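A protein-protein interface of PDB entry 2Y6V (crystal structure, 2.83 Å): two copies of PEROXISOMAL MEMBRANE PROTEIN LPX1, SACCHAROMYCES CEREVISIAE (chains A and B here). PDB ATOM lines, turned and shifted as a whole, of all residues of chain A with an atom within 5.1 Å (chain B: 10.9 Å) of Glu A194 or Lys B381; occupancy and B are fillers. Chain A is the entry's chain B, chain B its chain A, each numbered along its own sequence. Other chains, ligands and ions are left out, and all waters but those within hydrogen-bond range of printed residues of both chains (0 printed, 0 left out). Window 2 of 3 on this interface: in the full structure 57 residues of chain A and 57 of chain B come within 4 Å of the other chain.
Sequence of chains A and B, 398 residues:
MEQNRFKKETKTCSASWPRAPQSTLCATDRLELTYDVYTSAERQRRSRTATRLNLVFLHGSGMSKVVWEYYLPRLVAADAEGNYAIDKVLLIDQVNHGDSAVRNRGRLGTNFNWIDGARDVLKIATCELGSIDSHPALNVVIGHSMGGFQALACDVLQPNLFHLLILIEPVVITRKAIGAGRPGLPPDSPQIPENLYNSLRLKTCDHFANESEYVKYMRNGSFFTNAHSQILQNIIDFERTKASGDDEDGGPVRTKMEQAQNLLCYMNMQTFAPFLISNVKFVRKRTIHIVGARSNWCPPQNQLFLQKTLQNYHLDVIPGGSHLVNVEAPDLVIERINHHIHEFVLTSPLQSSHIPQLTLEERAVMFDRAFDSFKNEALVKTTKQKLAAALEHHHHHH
N of Ile A192 sits at hydrogen-bond distance from O of Ala B378, 2.7 Å away.
The backbone NH (N) of Glu A194 sits at hydrogen-bond distance from the backbone carbonyl oxygen (O) of Val B380, at 3.0 Å.
The backbone NH (N) of Val B380 sits at hydrogen-bond distance from the backbone carbonyl oxygen (O) of Ile A192 (2.8 Å).
The backbone carbonyl oxygen of Glu A194 sits at hydrogen-bond distance from the side-chain amide nitrogen of Asn A198.
Among the printed residues, pairs that only touch across the chains: Ile A192 with Leu B379 (3.5 Å), Pro A193 with Val B380 (3.7 Å), Glu A194 with Leu B379 (3.6 Å), Glu A194 with Lys B381 (3.1 Å), Tyr A197 with Lys B375 (3.5 Å) and Tyr A197 with Leu B379 (3.9 Å).
Glu A194 touches just these residues of chain B: Leu B379 (3.6 Å), Val B380 (3.0 Å) and Lys B381 (3.1 Å).
Lys B381 touches just one residue of chain A: Glu A194 (3.1 Å).
Pro A193 touches just one residue of chain B: Val B380.
No residue of chain B comes within 4 Å of Asn A195.
No residue of chain B comes within 4 Å of Asn A198.
Of the printed residues of chain B, Ile A192 touches Ala B378 (2.7 Å), Leu B379 (3.5 Å) and Val B380 (2.8 Å).
Printed residues of chain A within 4 Å of Ala B378: Ile A192.
Of the printed residues of chain A, Lys B375 touches Tyr A197.
Leu A196 touches none of the printed residues of chain B.
The nearest printed residue of chain A that does not touch Ala B378 is Pro A193 (5.1 Å).
Hydrophobic or aromatic side chains of chain A that line the printed part of chain B: Ile A192 and Tyr A197.
Of the 8 printed residues of chain B, 5 touch a printed residue of chain A.
Printed residues of chain B that touch a printed residue of chain A: Lys B375, Ala B378, Leu B379, Val B380 and Lys B381.
Along chain B the printed residues that touch a printed residue of chain A span positions 375 to 381.
Among the printed residues, 9 pairs touch across the chains.
Among the printed residues, no Asp or Glu carboxylate lies within 4 Å of a Lys or Arg side-chain nitrogen of the other chain.
No position is printed for both chains.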
ATOM      1  N   ILE A 178      11.204  33.939  22.293  1.00  0.00           N
ATOM      2  CA  ILE A 178      10.734  33.877  20.916  1.00  0.00           C
ATOM      3  C   ILE A 178       9.594  32.842  20.816  1.00  0.00           C
ATOM      4  O   ILE A 178       9.779  31.706  20.385  1.00  0.00           O
ATOM      5  CB  ILE A 178      11.921  33.618  19.929  1.00  0.00           C
ATOM      6  CG1 ILE A 178      13.054  34.650  20.167  1.00  0.00           C
ATOM      7  CG2 ILE A 178      11.454  33.679  18.460  1.00  0.00           C
ATOM      8  CD1 ILE A 178      14.318  34.487  19.200  1.00  0.00           C
ATOM      9  N   ILE A 192       9.410  30.802  30.671  1.00  0.00           N
ATOM     10  CA  ILE A 192      10.858  30.863  30.573  1.00  0.00           C
ATOM     11  C   ILE A 192      11.296  30.098  29.297  1.00  0.00           C
ATOM     12  O   ILE A 192      10.677  29.063  28.917  1.00  0.00           O
ATOM     13  CB  ILE A 192      11.547  30.256  31.801  1.00  0.00           C
ATOM     14  CG1 ILE A 192      13.011  30.678  31.839  1.00  0.00           C
ATOM     15  CG2 ILE A 192      11.484  28.749  31.786  1.00  0.00           C
ATOM     16  CD1 ILE A 192      13.673  30.514  33.220  1.00  0.00           C
ATOM     17  N   PRO A 193      12.321  30.623  28.596  1.00  0.00           N
ATOM     18  CA  PRO A 193      12.790  29.944  27.374  1.00  0.00           C
ATOM     19  C   PRO A 193      13.632  28.701  27.675  1.00  0.00           C
ATOM     20  O   PRO A 193      14.514  28.735  28.534  1.00  0.00           O
ATOM     21  CB  PRO A 193      13.632  31.012  26.652  1.00  0.00           C
ATOM     22  CG  PRO A 193      13.383  32.303  27.371  1.00  0.00           C
ATOM     23  CD  PRO A 193      12.832  32.001  28.720  1.00  0.00           C
ATOM     24  N   GLU A 194      13.373  27.611  26.966  1.00  0.00           N
ATOM     25  CA  GLU A 194      14.035  26.365  27.284  1.00  0.00           C
ATOM     26  C   GLU A 194      15.551  26.544  27.332  1.00  0.00           C
ATOM     27  O   GLU A 194      16.227  25.879  28.126  1.00  0.00           O
ATOM     28  CB  GLU A 194      13.688  25.271  26.274  1.00  0.00           C
ATOM     29  CG  GLU A 194      14.214  23.873  26.649  1.00  0.00           C
ATOM     30  CD  GLU A 194      13.759  22.784  25.678  1.00  0.00           C
ATOM     31  OE1 GLU A 194      12.999  23.120  24.749  1.00  0.00           O
ATOM     32  OE2 GLU A 194      14.154  21.598  25.838  1.00  0.00           O
ATOM     33  N   ASN A 195      16.103  27.403  26.470  1.00  0.00           N
ATOM     34  CA  ASN A 195      17.565  27.576  26.429  1.00  0.00           C
ATOM     35  C   ASN A 195      18.088  28.106  27.764  1.00  0.00           C
ATOM     36  O   ASN A 195      18.991  27.507  28.367  1.00  0.00           O
ATOM     37  CB  ASN A 195      17.998  28.438  25.228  1.00  0.00           C
ATOM     38  CG  ASN A 195      17.824  27.684  23.851  1.00  0.00           C
ATOM     39  OD1 ASN A 195      18.025  26.453  23.738  1.00  0.00           O
ATOM     40  ND2 ASN A 195      17.446  28.440  22.813  1.00  0.00           N
ATOM     41  N   LEU A 196      17.471  29.179  28.252  1.00  0.00           N
ATOM     42  CA  LEU A 196      17.865  29.808  29.510  1.00  0.00           C
ATOM     43  C   LEU A 196      17.692  28.821  30.666  1.00  0.00           C
ATOM     44  O   LEU A 196      18.543  28.765  31.542  1.00  0.00           O
ATOM     45  CB  LEU A 196      17.038  31.069  29.738  1.00  0.00           C
ATOM     46  CG  LEU A 196      17.368  31.919  30.967  1.00  0.00           C
ATOM     47  CD1 LEU A 196      18.801  32.416  30.929  1.00  0.00           C
ATOM     48  CD2 LEU A 196      16.346  33.089  31.113  1.00  0.00           C
ATOM     49  N   TYR A 197      16.614  28.023  30.657  1.00  0.00           N
ATOM     50  CA  TYR A 197      16.371  27.057  31.737  1.00  0.00           C
ATOM     51  C   TYR A 197      17.489  26.013  31.800  1.00  0.00           C
ATOM     52  O   TYR A 197      18.096  25.777  32.838  1.00  0.00           O
ATOM     53  CB  TYR A 197      15.015  26.375  31.570  1.00  0.00           C
ATOM     54  CG  TYR A 197      14.717  25.357  32.649  1.00  0.00           C
ATOM     55  CD1 TYR A 197      14.185  25.747  33.870  1.00  0.00           C
ATOM     56  CD2 TYR A 197      14.983  23.993  32.440  1.00  0.00           C
ATOM     57  CE1 TYR A 197      13.908  24.826  34.859  1.00  0.00           C
ATOM     58  CE2 TYR A 197      14.720  23.046  33.431  1.00  0.00           C
ATOM     59  CZ  TYR A 197      14.174  23.477  34.657  1.00  0.00           C
ATOM     60  OH  TYR A 197      13.891  22.572  35.688  1.00  0.00           O
ATOM     61  N   ASN A 198      17.788  25.413  30.662  1.00  0.00           N
ATOM     62  CA  ASN A 198      18.782  24.341  30.609  1.00  0.00           C
ATOM     63  C   ASN A 198      20.172  24.786  31.137  1.00  0.00           C
ATOM     64  O   ASN A 198      20.937  23.974  31.697  1.00  0.00           O
ATOM     65  CB  ASN A 198      18.917  23.787  29.183  1.00  0.00           C
ATOM     66  CG  ASN A 198      17.742  22.959  28.755  1.00  0.00           C
ATOM     67  OD1 ASN A 198      17.050  22.356  29.563  1.00  0.00           O
ATOM     68  ND2 ASN A 198      17.521  22.904  27.463  1.00  0.00           N
ATOM     69  N   ASP B 372       7.496  19.965  38.605  1.00  0.00           N
ATOM     70  CA  ASP B 372       7.469  19.431  37.266  1.00  0.00           C
ATOM     71  C   ASP B 372       6.291  19.925  36.453  1.00  0.00           C
ATOM     72  O   ASP B 372       6.494  20.331  35.322  1.00  0.00           O
ATOM     73  CB  ASP B 372       7.468  17.911  37.310  1.00  0.00           C
ATOM     74  CG  ASP B 372       8.860  17.313  37.072  1.00  0.00           C
ATOM     75  OD1 ASP B 372       9.885  17.956  37.412  1.00  0.00           O
ATOM     76  OD2 ASP B 372       8.930  16.186  36.514  1.00  0.00           O
ATOM     77  N   LYS B 375       7.051  23.524  35.636  1.00  0.00           N
ATOM     78  CA  LYS B 375       8.079  23.587  34.607  1.00  0.00           C
ATOM     79  C   LYS B 375       7.494  23.394  33.190  1.00  0.00           C
ATOM     80  O   LYS B 375       7.854  24.113  32.262  1.00  0.00           O
ATOM     81  CB  LYS B 375       9.171  22.544  34.882  1.00  0.00           C
ATOM     82  CG  LYS B 375      10.396  22.664  33.974  1.00  0.00           C
ATOM     83  CD  LYS B 375      11.214  21.383  33.858  1.00  0.00           C
ATOM     84  CE  LYS B 375      10.425  20.246  33.249  1.00  0.00           C
ATOM     85  NZ  LYS B 375      11.344  19.242  32.666  1.00  0.00           N
ATOM     86  N   ASN B 376       6.608  22.420  33.023  1.00  0.00           N
ATOM     87  CA  ASN B 376       6.040  22.148  31.702  1.00  0.00           C
ATOM     88  C   ASN B 376       5.131  23.276  31.194  1.00  0.00           C
ATOM     89  O   ASN B 376       5.118  23.562  29.993  1.00  0.00           O
ATOM     90  CB  ASN B 376       5.267  20.819  31.676  1.00  0.00           C
ATOM     91  CG  ASN B 376       6.174  19.577  31.812  1.00  0.00           C
ATOM     92  OD1 ASN B 376       7.406  19.616  31.653  1.00  0.00           O
ATOM     93  ND2 ASN B 376       5.536  18.453  32.106  1.00  0.00           N
ATOM     94  N   GLU B 377       4.367  23.901  32.093  1.00  0.00           N
ATOM     95  CA  GLU B 377       3.579  25.101  31.745  1.00  0.00           C
ATOM     96  C   GLU B 377       4.490  26.305  31.377  1.00  0.00           C
ATOM     97  O   GLU B 377       4.163  27.079  30.482  1.00  0.00           O
ATOM     98  CB  GLU B 377       2.668  25.538  32.909  1.00  0.00           C
ATOM     99  CG  GLU B 377       1.341  24.759  33.127  1.00  0.00           C
ATOM    100  CD  GLU B 377       0.557  25.247  34.399  1.00  0.00           C
ATOM    101  OE1 GLU B 377       1.210  25.603  35.426  1.00  0.00           O
ATOM    102  OE2 GLU B 377      -0.703  25.276  34.367  1.00  0.00           O
ATOM    103  N   ALA B 378       5.617  26.460  32.068  1.00  0.00           N
ATOM    104  CA  ALA B 378       6.443  27.651  31.920  1.00  0.00           C
ATOM    105  C   ALA B 378       7.468  27.559  30.793  1.00  0.00           C
ATOM    106  O   ALA B 378       7.910  28.573  30.272  1.00  0.00           O
ATOM    107  CB  ALA B 378       7.154  27.968  33.241  1.00  0.00           C
ATOM    108  N   LEU B 379       7.870  26.346  30.436  1.00  0.00           N
ATOM    109  CA  LEU B 379       8.887  26.148  29.398  1.00  0.00           C
ATOM    110  C   LEU B 379       8.418  26.525  27.985  1.00  0.00           C
ATOM    111  O   LEU B 379       7.363  26.065  27.525  1.00  0.00           O
ATOM    112  CB  LEU B 379       9.329  24.699  29.366  1.00  0.00           C
ATOM    113  CG  LEU B 379      10.539  24.349  30.210  1.00  0.00           C
ATOM    114  CD1 LEU B 379      10.826  22.860  30.056  1.00  0.00           C
ATOM    115  CD2 LEU B 379      11.738  25.160  29.792  1.00  0.00           C
ATOM    116  N   VAL B 380       9.231  27.336  27.300  1.00  0.00           N
ATOM    117  CA  VAL B 380       8.981  27.716  25.917  1.00  0.00           C
ATOM    118  C   VAL B 380      10.072  27.169  25.004  1.00  0.00           C
ATOM    119  O   VAL B 380      11.181  27.708  24.946  1.00  0.00           O
ATOM    120  CB  VAL B 380       8.914  29.233  25.783  1.00  0.00           C
ATOM    121  CG1 VAL B 380       8.589  29.625  24.346  1.00  0.00           C
ATOM    122  CG2 VAL B 380       7.884  29.796  26.767  1.00  0.00           C
ATOM    123  N   LYS B 381       9.736  26.101  24.280  1.00  0.00           N
ATOM    124  CA  LYS B 381      10.693  25.394  23.413  1.00  0.00           C
ATOM    125  C   LYS B 381      10.950  26.151  22.108  1.00  0.00           C
ATOM    126  O   LYS B 381      10.045  26.769  21.545  1.00  0.00           O
ATOM    127  CB  LYS B 381      10.192  23.970  23.118  1.00  0.00           C
ATOM    128  CG  LYS B 381       9.887  23.148  24.382  1.00  0.00           C
ATOM    129  CD  LYS B 381       9.480  21.700  24.082  1.00  0.00           C
ATOM    130  CE  LYS B 381       9.478  20.863  25.376  1.00  0.00           C
ATOM    131  NZ  LYS B 381       8.817  19.538  25.217  1.00  0.00           N
